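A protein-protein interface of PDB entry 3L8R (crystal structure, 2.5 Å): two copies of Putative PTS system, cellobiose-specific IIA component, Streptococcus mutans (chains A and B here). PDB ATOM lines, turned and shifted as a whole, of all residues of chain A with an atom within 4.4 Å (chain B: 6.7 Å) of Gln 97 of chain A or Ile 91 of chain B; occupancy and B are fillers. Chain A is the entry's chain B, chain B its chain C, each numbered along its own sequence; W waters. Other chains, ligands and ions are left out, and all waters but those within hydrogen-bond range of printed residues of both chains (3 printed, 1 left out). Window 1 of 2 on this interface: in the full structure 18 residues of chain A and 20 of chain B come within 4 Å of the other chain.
The side-chain amide nitrogen (NE2) of Gln 74 of chain A sits close to a ring nitrogen (ND1) of His 95 of chain B (3.4 Å).
The side-chain carboxylate (OD1) of Asp 98 of chain A lies close to the side-chain carboxylate (OD1) of Asp 98 of chain B (2.5 Å).
Of the 15 printed residues of chain A, 9 touch a printed residue of chain B.
Hydrophobic or aromatic side chains of chain A within 4 Å of the printed part of chain B: Leu 77, Leu 78, Tyr 81, Ile 89 and Met 101.
Asp 98 of chain A touches its own counterpart, Asp 98 of chain B.
6 positions are printed for both chains.
Of the printed residues of chain B, Ile 87 of chain A touches Glu 90.
His 95 of chain A touches none of the printed residues of chain B.
Of chain B, only Ile 91 (3.7 Å), Val 94 (3.4 Å) and Asp 98 (3.3 Å) come within 4 Å of Gln 97 of chain A.
Printed residues of chain B within 4 Å of Met 101 of chain A: His 95 and Asp 98.
Of chain A, only Leu 77 (3.8 Å), Tyr 81 (3.6 Å), Ile 89 (3.5 Å) and Gln 97 (3.7 Å) come within 4 Å of Ile 91 of chain B.
Ile 91 of chain B touches Leu 77 of chain A.
His 95 of chain B touches Leu 78 of chain A.
CB of Tyr 81 of chain A touches CG2 of Ile 91 of chain B, at 3.6 Å.
CG1 of Ile 92 of chain B touches CE2 of Tyr 81 of chain A, at 3.0 Å.
Glu 90 of chain B touches Ile 89 of chain A.
Ile 89 of chain A touches Ile 91 of chain B.
CG1 of Ile 91 of chain B touches NE2 of Gln 97 of chain A, at 3.7 Å.
Gln 97 of chain A touches Val 94 of chain B (OE1 to CG1, 3.4 Å).
Gln 97 of chain A touches Asp 98 of chain B.
CE of Met 101 of chain A touches CE1 of His 95 of chain B (3.7 Å).
The side-chain amide oxygen (OE1) of Gln 74 of chain A lies within hydrogen-bond range of the side-chain amide nitrogen (NE2) of Gln 97 of chain A, 3.2 Å away.
The side-chain sulfur (SD) of Met 101 of chain A lies within hydrogen-bond range of the side-chain amide nitrogen (NE2) of Gln 74 of chain A (3.6 Å).
Water W1 bridges the side-chain carboxylate (OE1) of Glu 90 of chain B and the backbone NH (N) of Ile 87 of chain A.
Water W3 lies within hydrogen-bond range of OE1 of Gln 74 of chain A, ND1 of His 95 of chain B, NE2 of Gln 97 of chain A and OD2 of Asp 98 of chain B.
Water W2 lies within hydrogen-bond range of the backbone carbonyl oxygen of Ile 87 of chain A (2.7 Å) and the side-chain carboxylate of Glu 90 of chain B (3.1 Å).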
ATOM      1  N   GLN A  74      -9.985   6.164   4.015  1.00  0.00           N
ATOM      2  CA  GLN A  74      -8.800   7.014   4.157  1.00  0.00           C
ATOM      3  C   GLN A  74      -8.893   8.233   3.266  1.00  0.00           C
ATOM      4  O   GLN A  74      -8.663   9.360   3.707  1.00  0.00           O
ATOM      5  CB  GLN A  74      -7.493   6.262   3.878  1.00  0.00           C
ATOM      6  CG  GLN A  74      -6.254   7.154   4.077  1.00  0.00           C
ATOM      7  CD  GLN A  74      -4.959   6.365   4.168  1.00  0.00           C
ATOM      8  OE1 GLN A  74      -4.447   6.140   5.256  1.00  0.00           O
ATOM      9  NE2 GLN A  74      -4.445   5.925   3.038  1.00  0.00           N
ATOM     10  N   LEU A  77     -11.219  10.849   4.547  1.00  0.00           N
ATOM     11  CA  LEU A  77     -10.527  11.472   5.667  1.00  0.00           C
ATOM     12  C   LEU A  77      -9.464  12.458   5.192  1.00  0.00           C
ATOM     13  O   LEU A  77      -9.348  13.559   5.734  1.00  0.00           O
ATOM     14  CB  LEU A  77      -9.889  10.378   6.506  1.00  0.00           C
ATOM     15  CG  LEU A  77     -10.245  10.320   7.962  1.00  0.00           C
ATOM     16  CD1 LEU A  77     -11.739  10.512   8.140  1.00  0.00           C
ATOM     17  CD2 LEU A  77      -9.778   8.950   8.418  1.00  0.00           C
ATOM     18  N   LEU A  78      -8.698  12.072   4.173  1.00  0.00           N
ATOM     19  CA  LEU A  78      -7.698  12.977   3.590  1.00  0.00           C
ATOM     20  C   LEU A  78      -8.359  14.200   2.922  1.00  0.00           C
ATOM     21  O   LEU A  78      -7.889  15.339   3.082  1.00  0.00           O
ATOM     22  CB  LEU A  78      -6.766  12.230   2.628  1.00  0.00           C
ATOM     23  CG  LEU A  78      -5.804  11.247   3.315  1.00  0.00           C
ATOM     24  CD1 LEU A  78      -5.259  10.180   2.376  1.00  0.00           C
ATOM     25  CD2 LEU A  78      -4.672  11.963   3.994  1.00  0.00           C
ATOM     26  N   TYR A  81      -9.538  16.855   5.541  1.00  0.00           N
ATOM     27  CA  TYR A  81      -8.399  17.601   5.992  1.00  0.00           C
ATOM     28  C   TYR A  81      -8.013  18.638   4.965  1.00  0.00           C
ATOM     29  O   TYR A  81      -7.860  19.812   5.300  1.00  0.00           O
ATOM     30  CB  TYR A  81      -7.200  16.673   6.262  1.00  0.00           C
ATOM     31  CG  TYR A  81      -5.970  17.444   6.612  1.00  0.00           C
ATOM     32  CD1 TYR A  81      -5.819  18.015   7.879  1.00  0.00           C
ATOM     33  CD2 TYR A  81      -4.969  17.662   5.659  1.00  0.00           C
ATOM     34  CE1 TYR A  81      -4.664  18.758   8.195  1.00  0.00           C
ATOM     35  CE2 TYR A  81      -3.846  18.412   5.955  1.00  0.00           C
ATOM     36  CZ  TYR A  81      -3.691  18.948   7.216  1.00  0.00           C
ATOM     37  OH  TYR A  81      -2.567  19.696   7.494  1.00  0.00           O
ATOM     38  N   ILE A  87      -8.711  17.570  11.978  1.00  0.00           N
ATOM     39  CA  ILE A  87      -8.714  16.158  12.308  1.00  0.00           C
ATOM     40  C   ILE A  87      -7.605  15.893  13.307  1.00  0.00           C
ATOM     41  O   ILE A  87      -6.432  16.015  13.002  1.00  0.00           O
ATOM     42  CB  ILE A  87      -8.489  15.297  11.075  1.00  0.00           C
ATOM     43  CG1 ILE A  87      -9.674  15.409  10.136  1.00  0.00           C
ATOM     44  CG2 ILE A  87      -8.290  13.846  11.487  1.00  0.00           C
ATOM     45  CD1 ILE A  87      -9.431  14.824   8.802  1.00  0.00           C
ATOM     46  N   ILE A  89      -5.443  13.585  15.409  1.00  0.00           N
ATOM     47  CA  ILE A  89      -5.007  12.243  15.087  1.00  0.00           C
ATOM     48  C   ILE A  89      -5.469  11.163  16.071  1.00  0.00           C
ATOM     49  O   ILE A  89      -6.614  10.633  15.909  1.00  0.00           O
ATOM     50  CB  ILE A  89      -3.537  12.175  14.583  1.00  0.00           C
ATOM     51  CG1 ILE A  89      -3.546  12.678  13.124  1.00  0.00           C
ATOM     52  CG2 ILE A  89      -2.970  10.763  14.628  1.00  0.00           C
ATOM     53  CD1 ILE A  89      -4.801  12.186  12.300  1.00  0.00           C
ATOM     54  N   MET A  93      -6.166   5.960  14.739  1.00  0.00           N
ATOM     55  CA  MET A  93      -6.028   6.380  13.337  1.00  0.00           C
ATOM     56  C   MET A  93      -4.689   5.929  12.728  1.00  0.00           C
ATOM     57  O   MET A  93      -4.672   5.226  11.718  1.00  0.00           O
ATOM     58  CB  MET A  93      -6.194   7.898  13.194  1.00  0.00           C
ATOM     59  CG  MET A  93      -6.525   8.310  11.772  1.00  0.00           C
ATOM     60  SD  MET A  93      -8.058   7.558  11.183  1.00  0.00           S
ATOM     61  CE  MET A  93      -7.473   6.781   9.727  1.00  0.00           C
ATOM     62  N   VAL A  94      -3.579   6.291  13.382  1.00  0.00           N
ATOM     63  CA  VAL A  94      -2.263   5.885  12.976  1.00  0.00           C
ATOM     64  C   VAL A  94      -2.258   4.403  12.701  1.00  0.00           C
ATOM     65  O   VAL A  94      -1.860   3.937  11.598  1.00  0.00           O
ATOM     66  CB  VAL A  94      -1.317   6.153  14.103  1.00  0.00           C
ATOM     67  CG1 VAL A  94       0.141   5.855  13.726  1.00  0.00           C
ATOM     68  CG2 VAL A  94      -1.488   7.582  14.594  1.00  0.00           C
ATOM     69  N   HIS A  95      -2.757   3.644  13.674  1.00  0.00           N
ATOM     70  CA  HIS A  95      -2.728   2.177  13.561  1.00  0.00           C
ATOM     71  C   HIS A  95      -3.548   1.663  12.428  1.00  0.00           C
ATOM     72  O   HIS A  95      -3.157   0.715  11.755  1.00  0.00           O
ATOM     73  CB  HIS A  95      -3.223   1.538  14.825  1.00  0.00           C
ATOM     74  CG  HIS A  95      -3.187   0.039  14.793  1.00  0.00           C
ATOM     75  ND1 HIS A  95      -2.023  -0.669  14.559  1.00  0.00           N
ATOM     76  CD2 HIS A  95      -4.158  -0.883  15.012  1.00  0.00           C
ATOM     77  CE1 HIS A  95      -2.280  -1.966  14.636  1.00  0.00           C
ATOM     78  NE2 HIS A  95      -3.565  -2.123  14.914  1.00  0.00           N
ATOM     79  N   ALA A  96      -4.694   2.293  12.214  1.00  0.00           N
ATOM     80  CA  ALA A  96      -5.497   2.042  11.029  1.00  0.00           C
ATOM     81  C   ALA A  96      -4.739   2.289   9.717  1.00  0.00           C
ATOM     82  O   ALA A  96      -4.673   1.401   8.817  1.00  0.00           O
ATOM     83  CB  ALA A  96      -6.702   2.911  11.063  1.00  0.00           C
ATOM     84  N   GLN A  97      -4.175   3.494   9.617  1.00  0.00           N
ATOM     85  CA  GLN A  97      -3.488   3.863   8.399  1.00  0.00           C
ATOM     86  C   GLN A  97      -2.394   2.875   8.166  1.00  0.00           C
ATOM     87  O   GLN A  97      -2.234   2.421   7.039  1.00  0.00           O
ATOM     88  CB  GLN A  97      -3.001   5.304   8.455  1.00  0.00           C
ATOM     89  CG  GLN A  97      -4.195   6.184   8.675  1.00  0.00           C
ATOM     90  CD  GLN A  97      -3.893   7.625   8.706  1.00  0.00           C
ATOM     91  OE1 GLN A  97      -3.946   8.243   9.769  1.00  0.00           O
ATOM     92  NE2 GLN A  97      -3.567   8.202   7.536  1.00  0.00           N
ATOM     93  N   ASP A  98      -1.714   2.438   9.222  1.00  0.00           N
ATOM     94  CA  ASP A  98      -0.602   1.561   9.003  1.00  0.00           C
ATOM     95  C   ASP A  98      -1.123   0.341   8.403  1.00  0.00           C
ATOM     96  O   ASP A  98      -0.561  -0.171   7.473  1.00  0.00           O
ATOM     97  CB  ASP A  98       0.102   1.185  10.287  1.00  0.00           C
ATOM     98  CG  ASP A  98       1.018   2.233  10.742  1.00  0.00           C
ATOM     99  OD1 ASP A  98       1.536   3.033   9.910  1.00  0.00           O
ATOM    100  OD2 ASP A  98       1.136   2.348  11.967  1.00  0.00           O
ATOM    101  N   HIS A  99      -2.204  -0.137   8.976  1.00  0.00           N
ATOM    102  CA  HIS A  99      -2.856  -1.349   8.553  1.00  0.00           C
ATOM    103  C   HIS A  99      -3.325  -1.290   7.115  1.00  0.00           C
ATOM    104  O   HIS A  99      -3.093  -2.261   6.391  1.00  0.00           O
ATOM    105  CB  HIS A  99      -4.019  -1.675   9.481  1.00  0.00           C
ATOM    106  CG  HIS A  99      -4.295  -3.130   9.564  1.00  0.00           C
ATOM    107  ND1 HIS A  99      -4.120  -3.845  10.725  1.00  0.00           N
ATOM    108  CD2 HIS A  99      -4.634  -4.029   8.599  1.00  0.00           C
ATOM    109  CE1 HIS A  99      -4.366  -5.124  10.476  1.00  0.00           C
ATOM    110  NE2 HIS A  99      -4.683  -5.263   9.195  1.00  0.00           N
ATOM    111  N   LEU A 100      -3.955  -0.187   6.673  1.00  0.00           N
ATOM    112  CA  LEU A 100      -4.332  -0.074   5.217  1.00  0.00           C
ATOM    113  C   LEU A 100      -3.116  -0.248   4.338  1.00  0.00           C
ATOM    114  O   LEU A 100      -3.029  -1.182   3.535  1.00  0.00           O
ATOM    115  CB  LEU A 100      -4.846   1.334   4.863  1.00  0.00           C
ATOM    116  CG  LEU A 100      -5.911   1.459   3.758  1.00  0.00           C
ATOM    117  CD1 LEU A 100      -6.013   2.895   3.271  1.00  0.00           C
ATOM    118  CD2 LEU A 100      -5.815   0.478   2.574  1.00  0.00           C
ATOM    119  N   MET A 101      -2.174   0.684   4.531  1.00  0.00           N
ATOM    120  CA  MET A 101      -1.075   0.946   3.628  1.00  0.00           C
ATOM    121  C   MET A 101      -0.102  -0.218   3.588  1.00  0.00           C
ATOM    122  O   MET A 101       0.487  -0.521   2.540  1.00  0.00           O
ATOM    123  CB  MET A 101      -0.356   2.181   4.136  1.00  0.00           C
ATOM    124  CG  MET A 101      -1.226   3.442   4.054  1.00  0.00           C
ATOM    125  SD  MET A 101      -1.518   3.897   2.304  1.00  0.00           S
ATOM    126  CE  MET A 101      -0.093   4.965   2.114  1.00  0.00           C
ATOM    127  N   ILE B  89       0.575  16.804  14.704  1.00  0.00           N
ATOM    128  CA  ILE B  89       0.700  15.764  13.711  1.00  0.00           C
ATOM    129  C   ILE B  89       0.055  15.942  12.394  1.00  0.00           C
ATOM    130  O   ILE B  89       0.746  16.272  11.409  1.00  0.00           O
ATOM    131  CB  ILE B  89       0.793  14.337  14.279  1.00  0.00           C
ATOM    132  CG1 ILE B  89       2.251  14.128  14.711  1.00  0.00           C
ATOM    133  CG2 ILE B  89       0.440  13.246  13.231  1.00  0.00           C
ATOM    134  CD1 ILE B  89       3.224  14.092  13.512  1.00  0.00           C
ATOM    135  N   GLU B  90      -1.243  15.817  12.346  1.00  0.00           N
ATOM    136  CA  GLU B  90      -1.912  15.908  11.062  1.00  0.00           C
ATOM    137  C   GLU B  90      -1.910  14.609  10.268  1.00  0.00           C
ATOM    138  O   GLU B  90      -0.876  13.999  10.025  1.00  0.00           O
ATOM    139  CB  GLU B  90      -1.368  17.056  10.195  1.00  0.00           C
ATOM    140  CG  GLU B  90      -1.560  18.473  10.785  1.00  0.00           C
ATOM    141  CD  GLU B  90      -2.843  18.628  11.605  1.00  0.00           C
ATOM    142  OE1 GLU B  90      -3.867  17.928  11.388  1.00  0.00           O
ATOM    143  OE2 GLU B  90      -2.807  19.457  12.503  1.00  0.00           O
ATOM    144  N   ILE B  91      -3.102  14.235   9.842  1.00  0.00           N
ATOM    145  CA  ILE B  91      -3.316  13.075   9.086  1.00  0.00           C
ATOM    146  C   ILE B  91      -2.497  12.979   7.790  1.00  0.00           C
ATOM    147  O   ILE B  91      -2.173  11.850   7.399  1.00  0.00           O
ATOM    148  CB  ILE B  91      -4.847  12.845   8.857  1.00  0.00           C
ATOM    149  CG1 ILE B  91      -5.098  11.479   8.206  1.00  0.00           C
ATOM    150  CG2 ILE B  91      -5.482  13.993   8.039  1.00  0.00           C
ATOM    151  CD1 ILE B  91      -6.524  11.095   8.117  1.00  0.00           C
ATOM    152  N   ILE B  92      -2.148  14.094   7.119  1.00  0.00           N
ATOM    153  CA  ILE B  92      -1.375  13.954   5.876  1.00  0.00           C
ATOM    154  C   ILE B  92       0.077  13.598   6.179  1.00  0.00           C
ATOM    155  O   ILE B  92       0.796  13.087   5.309  1.00  0.00           O
ATOM    156  CB  ILE B  92      -1.327  15.201   4.928  1.00  0.00           C
ATOM    157  CG1 ILE B  92      -1.487  16.522   5.667  1.00  0.00           C
ATOM    158  CG2 ILE B  92      -2.281  15.041   3.733  1.00  0.00           C
ATOM    159  CD1 ILE B  92      -0.328  16.861   6.565  1.00  0.00           C
ATOM    160  N   MET B  93       0.530  13.919   7.391  1.00  0.00           N
ATOM    161  CA  MET B  93       1.888  13.550   7.752  1.00  0.00           C
ATOM    162  C   MET B  93       1.912  12.057   7.966  1.00  0.00           C
ATOM    163  O   MET B  93       2.743  11.362   7.388  1.00  0.00           O
ATOM    164  CB  MET B  93       2.392  14.301   8.971  1.00  0.00           C
ATOM    165  CG  MET B  93       3.862  14.004   9.302  1.00  0.00           C
ATOM    166  SD  MET B  93       5.030  14.549   8.013  1.00  0.00           S
ATOM    167  CE  MET B  93       4.780  16.306   8.145  1.00  0.00           C
ATOM    168  N   VAL B  94       0.974  11.558   8.762  1.00  0.00           N
ATOM    169  CA  VAL B  94       0.824  10.119   8.990  1.00  0.00           C
ATOM    170  C   VAL B  94       0.835   9.465   7.642  1.00  0.00           C
ATOM    171  O   VAL B  94       1.583   8.492   7.398  1.00  0.00           O
ATOM    172  CB  VAL B  94      -0.507   9.804   9.621  1.00  0.00           C
ATOM    173  CG1 VAL B  94      -0.577   8.365   9.959  1.00  0.00           C
ATOM    174  CG2 VAL B  94      -0.707  10.704  10.890  1.00  0.00           C
ATOM    175  N   HIS B  95       0.070  10.044   6.727  1.00  0.00           N
ATOM    176  CA  HIS B  95      -0.011   9.454   5.396  1.00  0.00           C
ATOM    177  C   HIS B  95       1.295   9.546   4.587  1.00  0.00           C
ATOM    178  O   HIS B  95       1.719   8.589   3.971  1.00  0.00           O
ATOM    179  CB  HIS B  95      -1.168  10.057   4.666  1.00  0.00           C
ATOM    180  CG  HIS B  95      -1.386   9.491   3.317  1.00  0.00           C
ATOM    181  ND1 HIS B  95      -1.988   8.268   3.120  1.00  0.00           N
ATOM    182  CD2 HIS B  95      -1.132   9.999   2.090  1.00  0.00           C
ATOM    183  CE1 HIS B  95      -2.089   8.041   1.821  1.00  0.00           C
ATOM    184  NE2 HIS B  95      -1.574   9.074   1.174  1.00  0.00           N
ATOM    185  N   ALA B  96       1.967  10.672   4.640  1.00  0.00           N
ATOM    186  CA  ALA B  96       3.319  10.782   4.081  1.00  0.00           C
ATOM    187  C   ALA B  96       4.326   9.742   4.655  1.00  0.00           C
ATOM    188  O   ALA B  96       5.048   9.068   3.883  1.00  0.00           O
ATOM    189  CB  ALA B  96       3.873  12.270   4.195  1.00  0.00           C
ATOM    190  N   ASP B  98       3.625   6.910   6.152  1.00  0.00           N
ATOM    191  CA  ASP B  98       3.261   5.594   5.637  1.00  0.00           C
ATOM    192  C   ASP B  98       3.734   5.378   4.200  1.00  0.00           C
ATOM    193  O   ASP B  98       4.153   4.275   3.844  1.00  0.00           O
ATOM    194  CB  ASP B  98       1.761   5.380   5.670  1.00  0.00           C
ATOM    195  CG  ASP B  98       1.228   5.169   7.046  1.00  0.00           C
ATOM    196  OD1 ASP B  98       1.904   4.649   7.991  1.00  0.00           O
ATOM    197  OD2 ASP B  98       0.079   5.568   7.199  1.00  0.00           O
HETATM  198  O   HOH W   1      -5.901  19.146  11.770  1.00  0.00           O
HETATM  199  O   HOH W   2      -4.241  16.997  14.322  1.00  0.00           O
HETATM  200  O   HOH W   3      -2.077   6.846   5.382  1.00  0.00           O
